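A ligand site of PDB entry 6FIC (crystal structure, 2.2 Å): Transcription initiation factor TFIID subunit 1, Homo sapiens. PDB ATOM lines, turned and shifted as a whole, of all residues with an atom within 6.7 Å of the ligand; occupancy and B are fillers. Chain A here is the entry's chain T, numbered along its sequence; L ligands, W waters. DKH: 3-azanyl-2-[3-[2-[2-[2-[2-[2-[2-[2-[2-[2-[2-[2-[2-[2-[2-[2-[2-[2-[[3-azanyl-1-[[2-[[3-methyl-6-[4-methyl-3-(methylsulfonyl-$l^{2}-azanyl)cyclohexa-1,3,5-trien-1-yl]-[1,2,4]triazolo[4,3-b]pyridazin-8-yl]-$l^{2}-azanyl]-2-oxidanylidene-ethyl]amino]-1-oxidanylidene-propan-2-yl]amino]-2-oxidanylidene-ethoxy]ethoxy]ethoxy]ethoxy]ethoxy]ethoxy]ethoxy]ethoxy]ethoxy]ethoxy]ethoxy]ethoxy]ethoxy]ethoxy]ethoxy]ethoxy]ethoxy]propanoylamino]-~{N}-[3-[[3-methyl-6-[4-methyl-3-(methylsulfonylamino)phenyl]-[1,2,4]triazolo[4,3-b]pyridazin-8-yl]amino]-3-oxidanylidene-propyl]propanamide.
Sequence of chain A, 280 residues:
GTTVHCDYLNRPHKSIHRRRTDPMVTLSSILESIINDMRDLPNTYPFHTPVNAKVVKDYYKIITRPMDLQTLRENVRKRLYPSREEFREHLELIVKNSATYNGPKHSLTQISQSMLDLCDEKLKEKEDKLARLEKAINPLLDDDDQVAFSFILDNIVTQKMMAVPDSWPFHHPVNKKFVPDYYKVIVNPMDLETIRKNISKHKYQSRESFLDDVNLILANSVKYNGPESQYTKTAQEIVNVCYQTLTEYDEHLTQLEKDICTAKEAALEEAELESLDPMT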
ATOM      1  N   TYR A  45      18.296   6.861  25.342  1.00  0.00           N
ATOM      2  CA  TYR A  45      18.410   6.022  24.124  1.00  0.00           C
ATOM      3  C   TYR A  45      17.454   4.867  23.959  1.00  0.00           C
ATOM      4  O   TYR A  45      17.106   4.571  22.801  1.00  0.00           O
ATOM      5  CB  TYR A  45      19.863   5.543  23.836  1.00  0.00           C
ATOM      6  CG  TYR A  45      20.361   4.556  24.864  1.00  0.00           C
ATOM      7  CD1 TYR A  45      20.957   5.007  26.046  1.00  0.00           C
ATOM      8  CD2 TYR A  45      20.222   3.179  24.681  1.00  0.00           C
ATOM      9  CE1 TYR A  45      21.397   4.102  27.026  1.00  0.00           C
ATOM     10  CE2 TYR A  45      20.658   2.272  25.651  1.00  0.00           C
ATOM     11  CZ  TYR A  45      21.251   2.743  26.788  1.00  0.00           C
ATOM     12  OH  TYR A  45      21.680   1.919  27.767  1.00  0.00           O
ATOM     13  N   PRO A  46      16.979   4.227  25.068  1.00  0.00           N
ATOM     14  CA  PRO A  46      16.011   3.119  24.791  1.00  0.00           C
ATOM     15  C   PRO A  46      14.710   3.587  24.179  1.00  0.00           C
ATOM     16  O   PRO A  46      14.031   2.791  23.508  1.00  0.00           O
ATOM     17  CB  PRO A  46      15.789   2.486  26.165  1.00  0.00           C
ATOM     18  CG  PRO A  46      17.037   2.729  26.901  1.00  0.00           C
ATOM     19  CD  PRO A  46      17.532   4.108  26.423  1.00  0.00           C
ATOM     20  N   PHE A  47      14.392   4.862  24.357  1.00  0.00           N
ATOM     21  CA  PHE A  47      13.173   5.440  23.838  1.00  0.00           C
ATOM     22  C   PHE A  47      13.388   6.157  22.515  1.00  0.00           C
ATOM     23  O   PHE A  47      12.426   6.651  21.963  1.00  0.00           O
ATOM     24  CB  PHE A  47      12.576   6.387  24.882  1.00  0.00           C
ATOM     25  CG  PHE A  47      12.419   5.767  26.189  1.00  0.00           C
ATOM     26  CD1 PHE A  47      11.507   4.764  26.366  1.00  0.00           C
ATOM     27  CD2 PHE A  47      13.202   6.113  27.228  1.00  0.00           C
ATOM     28  CE1 PHE A  47      11.391   4.130  27.597  1.00  0.00           C
ATOM     29  CE2 PHE A  47      13.082   5.500  28.456  1.00  0.00           C
ATOM     30  CZ  PHE A  47      12.186   4.512  28.626  1.00  0.00           C
ATOM     31  N   HIS A  48      14.635   6.216  22.006  1.00  0.00           N
ATOM     32  CA  HIS A  48      14.899   6.957  20.747  1.00  0.00           C
ATOM     33  C   HIS A  48      14.237   6.343  19.532  1.00  0.00           C
ATOM     34  O   HIS A  48      13.832   7.080  18.689  1.00  0.00           O
ATOM     35  CB  HIS A  48      16.403   7.203  20.491  1.00  0.00           C
ATOM     36  CG  HIS A  48      17.036   8.119  21.511  1.00  0.00           C
ATOM     37  ND1 HIS A  48      18.343   8.534  21.421  1.00  0.00           N
ATOM     38  CD2 HIS A  48      16.553   8.645  22.667  1.00  0.00           C
ATOM     39  CE1 HIS A  48      18.638   9.294  22.458  1.00  0.00           C
ATOM     40  NE2 HIS A  48      17.573   9.395  23.229  1.00  0.00           N
ATOM     41  N   THR A  49      14.161   5.012  19.425  1.00  0.00           N
ATOM     42  CA  THR A  49      13.688   4.346  18.207  1.00  0.00           C
ATOM     43  C   THR A  49      12.703   3.269  18.639  1.00  0.00           C
ATOM     44  O   THR A  49      12.627   2.924  19.825  1.00  0.00           O
ATOM     45  CB  THR A  49      14.854   3.684  17.429  1.00  0.00           C
ATOM     46  OG1 THR A  49      15.566   2.754  18.297  1.00  0.00           O
ATOM     47  CG2 THR A  49      15.890   4.745  16.961  1.00  0.00           C
ATOM     48  N   PRO A  50      11.936   2.737  17.693  1.00  0.00           N
ATOM     49  CA  PRO A  50      11.061   1.646  18.056  1.00  0.00           C
ATOM     50  C   PRO A  50      11.793   0.465  18.727  1.00  0.00           C
ATOM     51  O   PRO A  50      12.927   0.163  18.388  1.00  0.00           O
ATOM     52  CB  PRO A  50      10.461   1.191  16.705  1.00  0.00           C
ATOM     53  CG  PRO A  50      10.576   2.377  15.781  1.00  0.00           C
ATOM     54  CD  PRO A  50      11.865   3.077  16.258  1.00  0.00           C
ATOM     55  N   VAL A  51      11.108  -0.238  19.610  1.00  0.00           N
ATOM     56  CA  VAL A  51      11.689  -1.365  20.258  1.00  0.00           C
ATOM     57  C   VAL A  51      12.119  -2.374  19.187  1.00  0.00           C
ATOM     58  O   VAL A  51      11.367  -2.734  18.321  1.00  0.00           O
ATOM     59  CB  VAL A  51      10.789  -1.944  21.354  1.00  0.00           C
ATOM     60  CG1 VAL A  51      11.232  -3.367  21.739  1.00  0.00           C
ATOM     61  CG2 VAL A  51      10.901  -1.086  22.597  1.00  0.00           C
ATOM     62  N   ASN A  52      13.327  -2.880  19.311  1.00  0.00           N
ATOM     63  CA  ASN A  52      13.757  -4.085  18.576  1.00  0.00           C
ATOM     64  C   ASN A  52      13.476  -5.292  19.539  1.00  0.00           C
ATOM     65  O   ASN A  52      14.127  -5.467  20.559  1.00  0.00           O
ATOM     66  CB  ASN A  52      15.257  -3.972  18.346  1.00  0.00           C
ATOM     67  CG  ASN A  52      15.864  -5.143  17.554  1.00  0.00           C
ATOM     68  OD1 ASN A  52      15.408  -6.287  17.653  1.00  0.00           O
ATOM     69  ND2 ASN A  52      16.951  -4.867  16.825  1.00  0.00           N
ATOM     70  N   ALA A  53      12.565  -6.128  19.138  1.00  0.00           N
ATOM     71  CA  ALA A  53      12.073  -7.242  19.922  1.00  0.00           C
ATOM     72  C   ALA A  53      13.143  -8.292  20.160  1.00  0.00           C
ATOM     73  O   ALA A  53      13.029  -9.041  21.121  1.00  0.00           O
ATOM     74  CB  ALA A  53      10.884  -7.886  19.195  1.00  0.00           C
ATOM     75  N   VAL A  55      16.025  -7.606  21.225  1.00  0.00           N
ATOM     76  CA  VAL A  55      16.772  -7.118  22.370  1.00  0.00           C
ATOM     77  C   VAL A  55      15.890  -6.822  23.557  1.00  0.00           C
ATOM     78  O   VAL A  55      16.383  -6.609  24.636  1.00  0.00           O
ATOM     79  CB  VAL A  55      17.587  -5.872  21.837  1.00  0.00           C
ATOM     80  CG1 VAL A  55      17.890  -4.883  22.883  1.00  0.00           C
ATOM     81  CG2 VAL A  55      18.885  -6.360  21.239  1.00  0.00           C
ATOM     82  N   VAL A  56      14.592  -6.718  23.344  1.00  0.00           N
ATOM     83  CA  VAL A  56      13.647  -6.415  24.412  1.00  0.00           C
ATOM     84  C   VAL A  56      12.539  -7.498  24.319  1.00  0.00           C
ATOM     85  O   VAL A  56      11.542  -7.431  23.546  1.00  0.00           O
ATOM     86  CB  VAL A  56      13.050  -5.010  24.309  1.00  0.00           C
ATOM     87  CG1 VAL A  56      12.225  -4.702  25.528  1.00  0.00           C
ATOM     88  CG2 VAL A  56      14.134  -3.967  24.128  1.00  0.00           C
ATOM     89  N   TYR A  59       8.410  -7.751  23.877  1.00  0.00           N
ATOM     90  CA  TYR A  59       7.923  -6.430  24.019  1.00  0.00           C
ATOM     91  C   TYR A  59       6.616  -6.262  23.347  1.00  0.00           C
ATOM     92  O   TYR A  59       5.677  -5.741  23.943  1.00  0.00           O
ATOM     93  CB  TYR A  59       8.927  -5.370  23.476  1.00  0.00           C
ATOM     94  CG  TYR A  59       8.493  -3.980  23.835  1.00  0.00           C
ATOM     95  CD1 TYR A  59       8.769  -3.490  25.089  1.00  0.00           C
ATOM     96  CD2 TYR A  59       7.780  -3.200  22.941  1.00  0.00           C
ATOM     97  CE1 TYR A  59       8.413  -2.220  25.464  1.00  0.00           C
ATOM     98  CE2 TYR A  59       7.349  -1.895  23.314  1.00  0.00           C
ATOM     99  CZ  TYR A  59       7.652  -1.423  24.573  1.00  0.00           C
ATOM    100  OH  TYR A  59       7.298  -0.167  25.014  1.00  0.00           O
ATOM    101  N   MET A  67       5.210   3.282  21.295  1.00  0.00           N
ATOM    102  CA  MET A  67       5.540   4.640  20.857  1.00  0.00           C
ATOM    103  C   MET A  67       6.983   4.880  21.246  1.00  0.00           C
ATOM    104  O   MET A  67       7.500   4.291  22.195  1.00  0.00           O
ATOM    105  CB  MET A  67       4.612   5.667  21.507  1.00  0.00           C
ATOM    106  CG  MET A  67       4.855   7.101  21.042  1.00  0.00           C
ATOM    107  SD  MET A  67       4.796   7.347  19.266  1.00  0.00           S
ATOM    108  CE  MET A  67       3.215   6.744  18.755  1.00  0.00           C
ATOM    109  N   ASP A  68       7.657   5.712  20.451  1.00  0.00           N
ATOM    110  CA  ASP A  68       9.055   6.083  20.682  1.00  0.00           C
ATOM    111  C   ASP A  68       9.292   7.440  19.986  1.00  0.00           C
ATOM    112  O   ASP A  68       8.405   7.933  19.259  1.00  0.00           O
ATOM    113  CB  ASP A  68       9.947   5.025  20.071  1.00  0.00           C
ATOM    114  CG  ASP A  68       9.798   4.993  18.549  1.00  0.00           C
ATOM    115  OD1 ASP A  68       8.874   4.312  18.028  1.00  0.00           O
ATOM    116  OD2 ASP A  68      10.585   5.700  17.867  1.00  0.00           O
ATOM    117  N   ILE A  94       4.703   6.749  25.897  1.00  0.00           N
ATOM    118  CA  ILE A  94       6.050   6.207  26.055  1.00  0.00           C
ATOM    119  C   ILE A  94       6.255   5.867  27.528  1.00  0.00           C
ATOM    120  O   ILE A  94       6.815   4.801  27.883  1.00  0.00           O
ATOM    121  CB  ILE A  94       7.165   7.195  25.540  1.00  0.00           C
ATOM    122  CG1 ILE A  94       6.996   7.473  24.044  1.00  0.00           C
ATOM    123  CG2 ILE A  94       8.557   6.660  25.809  1.00  0.00           C
ATOM    124  CD1 ILE A  94       8.028   8.451  23.442  1.00  0.00           C
ATOM    125  N   ASN A  97       3.864   2.946  28.625  1.00  0.00           N
ATOM    126  CA  ASN A  97       4.368   1.687  28.121  1.00  0.00           C
ATOM    127  C   ASN A  97       5.577   1.243  28.932  1.00  0.00           C
ATOM    128  O   ASN A  97       5.715   0.074  29.205  1.00  0.00           O
ATOM    129  CB  ASN A  97       4.697   1.705  26.639  1.00  0.00           C
ATOM    130  CG  ASN A  97       3.496   1.792  25.741  1.00  0.00           C
ATOM    131  OD1 ASN A  97       2.367   1.456  26.076  1.00  0.00           O
ATOM    132  ND2 ASN A  97       3.752   2.195  24.514  1.00  0.00           N
ATOM    133  N   SER A  98       6.414   2.139  29.379  1.00  0.00           N
ATOM    134  CA  SER A  98       7.503   1.718  30.206  1.00  0.00           C
ATOM    135  C   SER A  98       6.983   1.259  31.577  1.00  0.00           C
ATOM    136  O   SER A  98       7.596   0.402  32.176  1.00  0.00           O
ATOM    137  CB  SER A  98       8.535   2.809  30.421  1.00  0.00           C
ATOM    138  OG  SER A  98       9.622   2.339  31.193  1.00  0.00           O
ATOM    139  N   TYR A 101       5.655  -2.283  31.000  1.00  0.00           N
ATOM    140  CA  TYR A 101       6.589  -3.346  30.676  1.00  0.00           C
ATOM    141  C   TYR A 101       7.622  -3.538  31.770  1.00  0.00           C
ATOM    142  O   TYR A 101       7.958  -4.637  32.091  1.00  0.00           O
ATOM    143  CB  TYR A 101       7.262  -3.088  29.353  1.00  0.00           C
ATOM    144  CG  TYR A 101       8.206  -4.133  28.915  1.00  0.00           C
ATOM    145  CD1 TYR A 101       7.763  -5.249  28.242  1.00  0.00           C
ATOM    146  CD2 TYR A 101       9.555  -4.003  29.164  1.00  0.00           C
ATOM    147  CE1 TYR A 101       8.659  -6.216  27.796  1.00  0.00           C
ATOM    148  CE2 TYR A 101      10.461  -4.995  28.752  1.00  0.00           C
ATOM    149  CZ  TYR A 101      10.015  -6.089  28.075  1.00  0.00           C
ATOM    150  OH  TYR A 101      10.898  -7.039  27.598  1.00  0.00           O
ATOM    151  N   ASN A 102       8.179  -2.481  32.297  1.00  0.00           N
ATOM    152  CA  ASN A 102       9.264  -2.566  33.257  1.00  0.00           C
ATOM    153  C   ASN A 102       8.822  -2.364  34.727  1.00  0.00           C
ATOM    154  O   ASN A 102       9.639  -2.590  35.613  1.00  0.00           O
ATOM    155  CB  ASN A 102      10.226  -1.395  32.966  1.00  0.00           C
ATOM    156  CG  ASN A 102      10.859  -1.475  31.601  1.00  0.00           C
ATOM    157  OD1 ASN A 102      11.517  -2.447  31.313  1.00  0.00           O
ATOM    158  ND2 ASN A 102      10.686  -0.435  30.783  1.00  0.00           N
ATOM    159  N   HIS A 106      10.446   1.521  37.922  1.00  0.00           N
ATOM    160  CA  HIS A 106      11.685   1.144  37.227  1.00  0.00           C
ATOM    161  C   HIS A 106      12.448   2.389  36.745  1.00  0.00           C
ATOM    162  O   HIS A 106      11.884   3.446  36.393  1.00  0.00           O
ATOM    163  CB  HIS A 106      11.390   0.218  36.070  1.00  0.00           C
ATOM    164  CG  HIS A 106      12.592  -0.499  35.590  1.00  0.00           C
ATOM    165  ND1 HIS A 106      13.604   0.117  34.889  1.00  0.00           N
ATOM    166  CD2 HIS A 106      12.947  -1.805  35.716  1.00  0.00           C
ATOM    167  CE1 HIS A 106      14.550  -0.768  34.625  1.00  0.00           C
ATOM    168  NE2 HIS A 106      14.169  -1.939  35.122  1.00  0.00           N
ATOM    169  N   LEU A 108      13.879   2.921  34.023  1.00  0.00           N
ATOM    170  CA  LEU A 108      13.553   3.325  32.666  1.00  0.00           C
ATOM    171  C   LEU A 108      12.302   4.181  32.675  1.00  0.00           C
ATOM    172  O   LEU A 108      12.187   5.115  31.900  1.00  0.00           O
ATOM    173  CB  LEU A 108      13.379   2.125  31.753  1.00  0.00           C
ATOM    174  CG  LEU A 108      14.704   1.436  31.354  1.00  0.00           C
ATOM    175  CD1 LEU A 108      14.350   0.120  30.697  1.00  0.00           C
ATOM    176  CD2 LEU A 108      15.543   2.279  30.414  1.00  0.00           C
HETATM  177  C1  DKH L   1      13.841  -2.144  28.119  1.00  0.00           C
HETATM  178  C2  DKH L   1      15.003  -2.122  27.356  1.00  0.00           C
HETATM  179  C6  DKH L   1      11.674   1.042  25.120  1.00  0.00           C
HETATM  180  C3  DKH L   1      15.107  -1.360  26.171  1.00  0.00           C
HETATM  181  C5  DKH L   1      11.846   0.126  26.281  1.00  0.00           C
HETATM  182  C10 DKH L   1      18.596  -1.282  23.666  1.00  0.00           C
HETATM  183  C4  DKH L   1      12.757  -1.331  27.659  1.00  0.00           C
HETATM  184  C7  DKH L   1      16.315  -1.381  25.314  1.00  0.00           C
HETATM  185  C8  DKH L   1      17.558  -1.683  25.830  1.00  0.00           C
HETATM  186  C16 DKH L   1      15.223  -4.971  32.034  1.00  0.00           C
HETATM  187  C15 DKH L   1      14.031  -4.545  31.146  1.00  0.00           C
HETATM  188  C17 DKH L   1      16.714  -3.917  33.740  1.00  0.00           C
HETATM  189  C14 DKH L   1      19.777  -1.488  22.745  1.00  0.00           C
HETATM  190  C18 DKH L   1      16.349  -4.681  34.995  1.00  0.00           C
HETATM  191  C13 DKH L   1      15.080   0.862  21.144  1.00  0.00           C
HETATM  192  C12 DKH L   1      16.228  -1.006  23.976  1.00  0.00           C
HETATM  193  O3  DKH L   1      17.778  -3.326  33.639  1.00  0.00           O
HETATM  194  N6  DKH L   1      15.773  -3.843  32.797  1.00  0.00           N
HETATM  195  C   DKH L   1      14.440  -3.800  29.879  1.00  0.00           C
HETATM  196  O   DKH L   1      15.503  -4.036  29.349  1.00  0.00           O
HETATM  197  N   DKH L   1      13.590  -2.872  29.327  1.00  0.00           N
HETATM  198  N3  DKH L   1      11.539  -1.059  28.097  1.00  0.00           N
HETATM  199  N4  DKH L   1      10.987  -0.118  27.225  1.00  0.00           N
HETATM  200  N2  DKH L   1      12.982  -0.605  26.524  1.00  0.00           N
HETATM  201  N1  DKH L   1      14.123  -0.593  25.739  1.00  0.00           N
HETATM  202  C11 DKH L   1      17.351  -0.941  23.166  1.00  0.00           C
HETATM  203  N5  DKH L   1      17.214  -0.661  21.787  1.00  0.00           N
HETATM  204  S   DKH L   1      15.921  -0.633  20.845  1.00  0.00           S
HETATM  205  O2  DKH L   1      16.359  -0.625  19.488  1.00  0.00           O
HETATM  206  O1  DKH L   1      15.096  -1.738  21.291  1.00  0.00           O
HETATM  207  C9  DKH L   1      18.683  -1.632  25.010  1.00  0.00           C
HETATM  208  O   HOH W   1      11.597   2.582  22.340  1.00  0.00           O
HETATM  209  O   HOH W   2      15.232   0.506  17.363  1.00  0.00           O
HETATM  210  O   HOH W   3       8.384   0.618  27.201  1.00  0.00           O
HETATM  211  O   HOH W   4      19.232   1.059  20.363  1.00  0.00           O
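ND2 of Asn 102 sits at hydrogen-bond distance from OG of Ser 98 (3.0 Å). ND1 of His 106 sits at hydrogen-bond distance from N of Leu 108, 2.9 Å away.
Water W2 lies within hydrogen-bond range of OG1 of Thr 49, O of Pro 50 and O2 of the ligand. Water W3 lies within hydrogen-bond range of OH of Tyr 59, N4 of the ligand, N of Ser 98 and O of Asn 97.
O of Pro 46 touches C13 of the ligand, 3.2 Å away. Phe 47 touches the ligand. OG1 of Thr 49 touches C13 of the ligand, at 3.5 Å. O of Pro 50 touches C13 of the ligand (3.6 Å). Val 51 touches the ligand. Val 55 touches the ligand. CG2 of Val 56 touches C3 of the ligand, 3.5 Å away. CE1 of Tyr 59 touches N4 of the ligand, 3.8 Å away. Tyr 101 touches the ligand. Leu 108 touches the ligand (CD1 to N, 3.4 Å). Of the 21 residues printed, 13 come within 4 Å of the ligand.
A nitrogen (N6) of the ligand sits at hydrogen-bond distance from a ring nitrogen (NE2) of His 106, at 3.4 Å. A nitrogen (N3) of the ligand lies within hydrogen-bond range of the side-chain amide nitrogen (ND2) of Asn 102 (2.9 Å). N of Asn 52 lies within hydrogen-bond range of O1 of the ligand, at 2.9 Å.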
